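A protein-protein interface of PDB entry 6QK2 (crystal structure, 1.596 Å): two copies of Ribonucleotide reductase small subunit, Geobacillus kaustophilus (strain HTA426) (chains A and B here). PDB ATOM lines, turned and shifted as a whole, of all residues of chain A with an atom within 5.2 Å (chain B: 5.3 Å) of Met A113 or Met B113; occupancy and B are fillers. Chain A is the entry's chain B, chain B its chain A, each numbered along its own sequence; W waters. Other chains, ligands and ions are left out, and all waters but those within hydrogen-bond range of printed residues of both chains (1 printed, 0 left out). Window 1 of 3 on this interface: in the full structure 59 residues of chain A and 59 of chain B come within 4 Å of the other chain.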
ATOM      1  N   THR A  87     -10.666   3.919 -28.723  1.00  0.00           N
ATOM      2  CA  THR A  87     -11.244   5.169 -29.226  1.00  0.00           C
ATOM      3  C   THR A  87     -11.822   4.970 -30.620  1.00  0.00           C
ATOM      4  O   THR A  87     -12.963   5.375 -30.897  1.00  0.00           O
ATOM      5  CB  THR A  87     -10.193   6.281 -29.237  1.00  0.00           C
ATOM      6  OG1 THR A  87      -9.712   6.484 -27.913  1.00  0.00           O
ATOM      7  CG2 THR A  87     -10.790   7.574 -29.709  1.00  0.00           C
ATOM      8  N   ILE A  90     -14.973   1.960 -30.789  1.00  0.00           N
ATOM      9  CA  ILE A  90     -16.307   2.077 -30.236  1.00  0.00           C
ATOM     10  C   ILE A  90     -17.296   2.601 -31.272  1.00  0.00           C
ATOM     11  O   ILE A  90     -18.505   2.451 -31.094  1.00  0.00           O
ATOM     12  CB  ILE A  90     -16.289   2.972 -28.984  1.00  0.00           C
ATOM     13  CG1 ILE A  90     -17.620   2.947 -28.231  1.00  0.00           C
ATOM     14  CG2 ILE A  90     -15.899   4.370 -29.350  1.00  0.00           C
ATOM     15  CD1 ILE A  90     -17.894   1.589 -27.554  1.00  0.00           C
ATOM     16  N   LEU A  91     -16.811   3.213 -32.357  1.00  0.00           N
ATOM     17  CA  LEU A  91     -17.729   3.839 -33.307  1.00  0.00           C
ATOM     18  C   LEU A  91     -18.743   2.866 -33.901  1.00  0.00           C
ATOM     19  O   LEU A  91     -19.906   3.262 -34.060  1.00  0.00           O
ATOM     20  CB  LEU A  91     -16.927   4.536 -34.416  1.00  0.00           C
ATOM     21  CG  LEU A  91     -16.129   5.751 -33.948  1.00  0.00           C
ATOM     22  CD1 LEU A  91     -15.162   6.212 -35.038  1.00  0.00           C
ATOM     23  CD2 LEU A  91     -17.112   6.855 -33.588  1.00  0.00           C
ATOM     24  N   ALA A  94     -21.651   2.448 -31.414  1.00  0.00           N
ATOM     25  CA  ALA A  94     -22.512   3.616 -31.409  1.00  0.00           C
ATOM     26  C   ALA A  94     -23.416   3.617 -32.630  1.00  0.00           C
ATOM     27  O   ALA A  94     -24.613   3.889 -32.525  1.00  0.00           O
ATOM     28  CB  ALA A  94     -21.664   4.883 -31.350  1.00  0.00           C
ATOM     29  N   LEU A 109     -22.922   6.940 -25.066  1.00  0.00           N
ATOM     30  CA  LEU A 109     -21.703   6.576 -25.766  1.00  0.00           C
ATOM     31  C   LEU A 109     -20.906   7.802 -26.214  1.00  0.00           C
ATOM     32  O   LEU A 109     -19.696   7.685 -26.419  1.00  0.00           O
ATOM     33  CB  LEU A 109     -22.004   5.646 -26.929  1.00  0.00           C
ATOM     34  CG  LEU A 109     -22.269   4.191 -26.480  1.00  0.00           C
ATOM     35  CD1 LEU A 109     -22.650   3.356 -27.690  1.00  0.00           C
ATOM     36  CD2 LEU A 109     -21.109   3.532 -25.712  1.00  0.00           C
ATOM     37  N   THR A 110     -21.533   8.975 -26.379  1.00  0.00           N
ATOM     38  CA  THR A 110     -20.722  10.154 -26.677  1.00  0.00           C
ATOM     39  C   THR A 110     -19.763  10.450 -25.519  1.00  0.00           C
ATOM     40  O   THR A 110     -18.660  10.932 -25.760  1.00  0.00           O
ATOM     41  CB  THR A 110     -21.572  11.399 -26.998  1.00  0.00           C
ATOM     42  OG1 THR A 110     -22.239  11.906 -25.836  1.00  0.00           O
ATOM     43  CG2 THR A 110     -22.585  11.130 -28.088  1.00  0.00           C
ATOM     44  N   THR A 111     -20.166  10.183 -24.266  1.00  0.00           N
ATOM     45  CA  THR A 111     -19.277  10.416 -23.127  1.00  0.00           C
ATOM     46  C   THR A 111     -18.216   9.329 -23.036  1.00  0.00           C
ATOM     47  O   THR A 111     -17.072   9.606 -22.665  1.00  0.00           O
ATOM     48  CB  THR A 111     -20.038  10.497 -21.787  1.00  0.00           C
ATOM     49  OG1 THR A 111     -20.501   9.213 -21.368  1.00  0.00           O
ATOM     50  CG2 THR A 111     -21.184  11.463 -21.848  1.00  0.00           C
ATOM     51  N   PHE A 112     -18.583   8.103 -23.409  1.00  0.00           N
ATOM     52  CA  PHE A 112     -17.641   6.993 -23.478  1.00  0.00           C
ATOM     53  C   PHE A 112     -16.531   7.316 -24.481  1.00  0.00           C
ATOM     54  O   PHE A 112     -15.330   7.249 -24.175  1.00  0.00           O
ATOM     55  CB  PHE A 112     -18.471   5.753 -23.849  1.00  0.00           C
ATOM     56  CG  PHE A 112     -17.792   4.421 -23.755  1.00  0.00           C
ATOM     57  CD1 PHE A 112     -18.445   3.379 -23.116  1.00  0.00           C
ATOM     58  CD2 PHE A 112     -16.593   4.152 -24.362  1.00  0.00           C
ATOM     59  CE1 PHE A 112     -17.913   2.124 -23.042  1.00  0.00           C
ATOM     60  CE2 PHE A 112     -16.027   2.867 -24.277  1.00  0.00           C
ATOM     61  CZ  PHE A 112     -16.698   1.858 -23.624  1.00  0.00           C
ATOM     62  N   MET A 113     -16.912   7.758 -25.674  1.00  0.00           N
ATOM     63  CA  MET A 113     -15.931   8.043 -26.718  1.00  0.00           C
ATOM     64  C   MET A 113     -15.032   9.211 -26.328  1.00  0.00           C
ATOM     65  O   MET A 113     -13.806   9.189 -26.552  1.00  0.00           O
ATOM     66  CB  MET A 113     -16.668   8.331 -28.028  1.00  0.00           C
ATOM     67  CG  MET A 113     -17.409   7.139 -28.482  1.00  0.00           C
ATOM     68  SD  MET A 113     -17.999   7.132 -30.178  1.00  0.00           S
ATOM     69  CE  MET A 113     -19.219   8.351 -29.950  1.00  0.00           C
ATOM     70  N   HIS A 114     -15.627  10.264 -25.781  1.00  0.00           N
ATOM     71  CA  HIS A 114     -14.820  11.393 -25.379  1.00  0.00           C
ATOM     72  C   HIS A 114     -13.875  11.004 -24.245  1.00  0.00           C
ATOM     73  O   HIS A 114     -12.734  11.478 -24.205  1.00  0.00           O
ATOM     74  CB  HIS A 114     -15.671  12.588 -24.982  1.00  0.00           C
ATOM     75  CG  HIS A 114     -14.828  13.739 -24.554  1.00  0.00           C
ATOM     76  ND1 HIS A 114     -13.853  14.262 -25.375  1.00  0.00           N
ATOM     77  CD2 HIS A 114     -14.715  14.386 -23.368  1.00  0.00           C
ATOM     78  CE1 HIS A 114     -13.203  15.218 -24.729  1.00  0.00           C
ATOM     79  NE2 HIS A 114     -13.723  15.328 -23.514  1.00  0.00           N
ATOM     80  N   ASP A 115     -14.331  10.162 -23.310  1.00  0.00           N
ATOM     81  CA  ASP A 115     -13.432   9.650 -22.261  1.00  0.00           C
ATOM     82  C   ASP A 115     -12.212   8.991 -22.892  1.00  0.00           C
ATOM     83  O   ASP A 115     -11.074   9.263 -22.488  1.00  0.00           O
ATOM     84  CB  ASP A 115     -14.130   8.618 -21.354  1.00  0.00           C
ATOM     85  CG  ASP A 115     -15.180   9.210 -20.410  1.00  0.00           C
ATOM     86  OD1 ASP A 115     -15.265  10.446 -20.255  1.00  0.00           O
ATOM     87  OD2 ASP A 115     -15.925   8.361 -19.855  1.00  0.00           O
ATOM     88  N   GLU A 116     -12.426   8.088 -23.859  1.00  0.00           N
ATOM     89  CA  GLU A 116     -11.283   7.376 -24.448  1.00  0.00           C
ATOM     90  C   GLU A 116     -10.328   8.346 -25.136  1.00  0.00           C
ATOM     91  O   GLU A 116      -9.112   8.164 -25.072  1.00  0.00           O
ATOM     92  CB  GLU A 116     -11.748   6.307 -25.430  1.00  0.00           C
ATOM     93  CG  GLU A 116     -12.694   5.249 -24.878  1.00  0.00           C
ATOM     94  CD  GLU A 116     -12.163   4.410 -23.748  1.00  0.00           C
ATOM     95  OE1 GLU A 116     -11.058   4.623 -23.238  1.00  0.00           O
ATOM     96  OE2 GLU A 116     -12.894   3.530 -23.333  1.00  0.00           O
ATOM     97  N   ALA A 117     -10.849   9.374 -25.803  1.00  0.00           N
ATOM     98  CA  ALA A 117      -9.995  10.418 -26.377  1.00  0.00           C
ATOM     99  C   ALA A 117      -9.068  11.010 -25.337  1.00  0.00           C
ATOM    100  O   ALA A 117      -7.868  11.185 -25.575  1.00  0.00           O
ATOM    101  CB  ALA A 117     -10.865  11.522 -26.998  1.00  0.00           C
ATOM    102  N   THR B  87     -26.740  14.391 -34.215  1.00  0.00           N
ATOM    103  CA  THR B  87     -26.092  13.507 -33.242  1.00  0.00           C
ATOM    104  C   THR B  87     -25.847  12.134 -33.857  1.00  0.00           C
ATOM    105  O   THR B  87     -24.758  11.565 -33.742  1.00  0.00           O
ATOM    106  CB  THR B  87     -26.949  13.365 -31.983  1.00  0.00           C
ATOM    107  OG1 THR B  87     -27.126  14.630 -31.344  1.00  0.00           O
ATOM    108  CG2 THR B  87     -26.292  12.437 -30.969  1.00  0.00           C
ATOM    109  N   ILE B  90     -23.297  12.158 -37.401  1.00  0.00           N
ATOM    110  CA  ILE B  90     -21.877  12.455 -37.424  1.00  0.00           C
ATOM    111  C   ILE B  90     -21.035  11.189 -37.329  1.00  0.00           C
ATOM    112  O   ILE B  90     -19.861  11.219 -37.724  1.00  0.00           O
ATOM    113  CB  ILE B  90     -21.488  13.448 -36.316  1.00  0.00           C
ATOM    114  CG1 ILE B  90     -20.051  13.988 -36.491  1.00  0.00           C
ATOM    115  CG2 ILE B  90     -21.703  12.824 -34.971  1.00  0.00           C
ATOM    116  CD1 ILE B  90     -19.861  14.848 -37.745  1.00  0.00           C
ATOM    117  N   LEU B  91     -21.619  10.070 -36.894  1.00  0.00           N
ATOM    118  CA  LEU B  91     -20.828   8.858 -36.709  1.00  0.00           C
ATOM    119  C   LEU B  91     -20.120   8.403 -37.975  1.00  0.00           C
ATOM    120  O   LEU B  91     -18.964   7.971 -37.874  1.00  0.00           O
ATOM    121  CB  LEU B  91     -21.699   7.724 -36.149  1.00  0.00           C
ATOM    122  CG  LEU B  91     -22.164   7.991 -34.722  1.00  0.00           C
ATOM    123  CD1 LEU B  91     -23.250   7.017 -34.292  1.00  0.00           C
ATOM    124  CD2 LEU B  91     -20.972   7.869 -33.803  1.00  0.00           C
ATOM    125  N   ALA B  94     -16.869  10.438 -38.376  1.00  0.00           N
ATOM    126  CA  ALA B  94     -15.842   9.985 -37.453  1.00  0.00           C
ATOM    127  C   ALA B  94     -15.211   8.682 -37.930  1.00  0.00           C
ATOM    128  O   ALA B  94     -13.985   8.520 -37.867  1.00  0.00           O
ATOM    129  CB  ALA B  94     -16.435   9.819 -36.049  1.00  0.00           C
ATOM    130  N   LEU B 109     -13.734  15.162 -32.955  1.00  0.00           N
ATOM    131  CA  LEU B 109     -15.110  14.746 -33.197  1.00  0.00           C
ATOM    132  C   LEU B 109     -15.744  14.090 -31.974  1.00  0.00           C
ATOM    133  O   LEU B 109     -16.961  14.113 -31.860  1.00  0.00           O
ATOM    134  CB  LEU B 109     -15.198  13.832 -34.420  1.00  0.00           C
ATOM    135  CG  LEU B 109     -15.035  14.605 -35.747  1.00  0.00           C
ATOM    136  CD1 LEU B 109     -14.999  13.629 -36.915  1.00  0.00           C
ATOM    137  CD2 LEU B 109     -16.144  15.620 -35.990  1.00  0.00           C
ATOM    138  N   THR B 110     -14.980  13.577 -31.014  1.00  0.00           N
ATOM    139  CA  THR B 110     -15.647  13.090 -29.800  1.00  0.00           C
ATOM    140  C   THR B 110     -16.291  14.247 -29.046  1.00  0.00           C
ATOM    141  O   THR B 110     -17.356  14.064 -28.423  1.00  0.00           O
ATOM    142  CB  THR B 110     -14.703  12.310 -28.874  1.00  0.00           C
ATOM    143  OG1 THR B 110     -13.754  13.196 -28.257  1.00  0.00           O
ATOM    144  CG2 THR B 110     -13.953  11.244 -29.601  1.00  0.00           C
ATOM    145  N   THR B 111     -15.673  15.428 -29.074  1.00  0.00           N
ATOM    146  CA  THR B 111     -16.277  16.606 -28.448  1.00  0.00           C
ATOM    147  C   THR B 111     -17.470  17.102 -29.255  1.00  0.00           C
ATOM    148  O   THR B 111     -18.449  17.585 -28.672  1.00  0.00           O
ATOM    149  CB  THR B 111     -15.268  17.758 -28.249  1.00  0.00           C
ATOM    150  OG1 THR B 111     -14.952  18.435 -29.475  1.00  0.00           O
ATOM    151  CG2 THR B 111     -14.000  17.238 -27.587  1.00  0.00           C
ATOM    152  N   PHE B 112     -17.381  17.022 -30.583  1.00  0.00           N
ATOM    153  CA  PHE B 112     -18.467  17.421 -31.479  1.00  0.00           C
ATOM    154  C   PHE B 112     -19.717  16.595 -31.209  1.00  0.00           C
ATOM    155  O   PHE B 112     -20.801  17.142 -30.955  1.00  0.00           O
ATOM    156  CB  PHE B 112     -17.949  17.256 -32.914  1.00  0.00           C
ATOM    157  CG  PHE B 112     -18.791  17.843 -34.013  1.00  0.00           C
ATOM    158  CD1 PHE B 112     -18.208  18.666 -34.953  1.00  0.00           C
ATOM    159  CD2 PHE B 112     -20.090  17.475 -34.197  1.00  0.00           C
ATOM    160  CE1 PHE B 112     -18.936  19.164 -36.019  1.00  0.00           C
ATOM    161  CE2 PHE B 112     -20.818  17.967 -35.274  1.00  0.00           C
ATOM    162  CZ  PHE B 112     -20.247  18.817 -36.163  1.00  0.00           C
ATOM    163  N   MET B 113     -19.560  15.269 -31.144  1.00  0.00           N
ATOM    164  CA  MET B 113     -20.683  14.365 -30.893  1.00  0.00           C
ATOM    165  C   MET B 113     -21.283  14.588 -29.521  1.00  0.00           C
ATOM    166  O   MET B 113     -22.514  14.581 -29.340  1.00  0.00           O
ATOM    167  CB  MET B 113     -20.209  12.916 -31.032  1.00  0.00           C
ATOM    168  CG  MET B 113     -19.762  12.653 -32.425  1.00  0.00           C
ATOM    169  SD  MET B 113     -19.491  10.945 -32.946  1.00  0.00           S
ATOM    170  CE  MET B 113     -17.952  10.750 -32.185  1.00  0.00           C
ATOM    171  N   HIS B 114     -20.429  14.724 -28.520  1.00  0.00           N
ATOM    172  CA  HIS B 114     -20.950  14.951 -27.183  1.00  0.00           C
ATOM    173  C   HIS B 114     -21.672  16.290 -27.091  1.00  0.00           C
ATOM    174  O   HIS B 114     -22.686  16.373 -26.387  1.00  0.00           O
ATOM    175  CB  HIS B 114     -19.851  14.856 -26.139  1.00  0.00           C
ATOM    176  CG  HIS B 114     -20.375  15.064 -24.759  1.00  0.00           C
ATOM    177  ND1 HIS B 114     -21.352  14.244 -24.238  1.00  0.00           N
ATOM    178  CD2 HIS B 114     -20.193  16.061 -23.861  1.00  0.00           C
ATOM    179  CE1 HIS B 114     -21.699  14.688 -23.039  1.00  0.00           C
ATOM    180  NE2 HIS B 114     -21.009  15.788 -22.784  1.00  0.00           N
ATOM    181  N   ASP B 115     -21.189  17.340 -27.784  1.00  0.00           N
ATOM    182  CA  ASP B 115     -21.937  18.608 -27.838  1.00  0.00           C
ATOM    183  C   ASP B 115     -23.344  18.368 -28.377  1.00  0.00           C
ATOM    184  O   ASP B 115     -24.338  18.853 -27.811  1.00  0.00           O
ATOM    185  CB  ASP B 115     -21.238  19.668 -28.727  1.00  0.00           C
ATOM    186  CG  ASP B 115     -19.905  20.186 -28.161  1.00  0.00           C
ATOM    187  OD1 ASP B 115     -19.624  20.025 -26.960  1.00  0.00           O
ATOM    188  OD2 ASP B 115     -19.171  20.791 -28.958  1.00  0.00           O
ATOM    189  N   GLU B 116     -23.453  17.652 -29.509  1.00  0.00           N
ATOM    190  CA  GLU B 116     -24.772  17.451 -30.114  1.00  0.00           C
ATOM    191  C   GLU B 116     -25.685  16.687 -29.160  1.00  0.00           C
ATOM    192  O   GLU B 116     -26.879  16.966 -29.085  1.00  0.00           O
ATOM    193  CB  GLU B 116     -24.658  16.727 -31.448  1.00  0.00           C
ATOM    194  CG  GLU B 116     -23.758  17.400 -32.463  1.00  0.00           C
ATOM    195  CD  GLU B 116     -24.187  18.770 -32.915  1.00  0.00           C
ATOM    196  OE1 GLU B 116     -25.159  19.363 -32.399  1.00  0.00           O
ATOM    197  OE2 GLU B 116     -23.484  19.274 -33.784  1.00  0.00           O
ATOM    198  N   ALA B 117     -25.147  15.715 -28.422  1.00  0.00           N
ATOM    199  CA  ALA B 117     -25.940  15.021 -27.406  1.00  0.00           C
ATOM    200  C   ALA B 117     -26.520  16.012 -26.399  1.00  0.00           C
ATOM    201  O   ALA B 117     -27.713  15.944 -26.045  1.00  0.00           O
ATOM    202  CB  ALA B 117     -25.092  13.961 -26.702  1.00  0.00           C
ATOM    203  N   LYS B 118     -25.686  16.937 -25.912  1.00  0.00           N
ATOM    204  CA  LYS B 118     -26.195  17.964 -25.004  1.00  0.00           C
ATOM    205  C   LYS B 118     -27.239  18.844 -25.686  1.00  0.00           C
ATOM    206  O   LYS B 118     -28.156  19.336 -25.021  1.00  0.00           O
ATOM    207  CB  LYS B 118     -25.038  18.813 -24.460  1.00  0.00           C
ATOM    208  CG  LYS B 118     -24.130  18.026 -23.549  1.00  0.00           C
ATOM    209  CD  LYS B 118     -23.117  18.904 -22.820  1.00  0.00           C
ATOM    210  CE  LYS B 118     -22.256  19.733 -23.704  1.00  0.00           C
ATOM    211  NZ  LYS B 118     -21.151  20.374 -22.872  1.00  0.00           N
HETATM  212  O   HOH W   1     -18.216  11.562 -28.471  1.00  0.00           O
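ND1 of His B114 is in hydrogen-bond range of OG1 of Thr A110, at 3.0 Å.
The side-chain hydroxyl of Thr B110 lies within hydrogen-bond range of a ring nitrogen (ND1) of His A114, at 3.1 Å.
Among the printed residues, merely in contact across the chains: Leu A91 with Leu B91 (3.997 Å), Leu A91 with Ala B94 (3.8 Å), Ala A94 with Leu B91 (3.8 Å), Thr A110 with Met B113 (3.7 Å), Thr A110 with Ala B117 (3.6 Å), Thr A111 with His B114 (3.5 Å), Met A113 with Thr B110 (3.7 Å), Met A113 with Met B113 (3.5 Å), His A114 with Thr B111 (3.6 Å) and Ala A117 with Thr B110 (3.6 Å).
Ile A90 touches none of the printed residues of chain B.
Printed residues of chain B within 4 Å of Leu A91: Leu B91 (3.997 Å) and Ala B94 (3.8 Å).
Printed residues of chain B within 4 Å of Ala A94: Leu B91.
Printed residues of chain B within 4 Å of Thr A111: His B114 (3.5 Å).
Of the printed residues of chain B, His A114 touches Thr B110 (3.1 Å) and Thr B111 (3.6 Å).
Leu B109 touches none of the printed residues of chain A.
Of the printed residues of chain A, Thr B111 touches His A114.
Of the printed residues of chain A, Met B113 touches Thr A110 (3.7 Å) and Met A113 (3.5 Å).
The nearest printed residue of chain B that does not touch Met A113 is Leu B91 (4.3 Å).
The nearest printed residue of chain A that does not touch Met B113 is Leu A91 (4.2 Å).
Of the 13 printed residues of chain A, 7 touch a printed residue of chain B.
Hydrophobic or aromatic side chains of chain A within 4 Å of the printed part of chain B: Leu A91, Ala A94, Met A113, His A114 and Ala A117.
Of the 14 printed residues of chain B, 7 touch a printed residue of chain A.
Printed residues of chain B that touch a printed residue of chain A: Leu B91, Ala B94, Thr B110, Thr B111, Met B113, His B114 and Ala B117.
Hydrophobic or aromatic side chains of chain B that line the printed part of chain A: Leu B91, Ala B94, Met B113, His B114 and Ala B117.
Among the printed residues, 12 pairs touch across the chains.
Leu B91 touches its own counterpart, Leu A91.
Thr A110 touches His B114, and with the chains exchanged His A114 touches Thr B110.
Thr A110 touches Ala B117, and with the chains exchanged Ala A117 touches Thr B110.
Met A113 touches its own counterpart, Met B113.
Of the 12 pairs that touch across the chains among the printed residues, 12 have their exchanged pair printed and touching as well.
Water W1 bridges O of Thr B110 (2.6 Å) and O of Thr A110 (2.8 Å).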
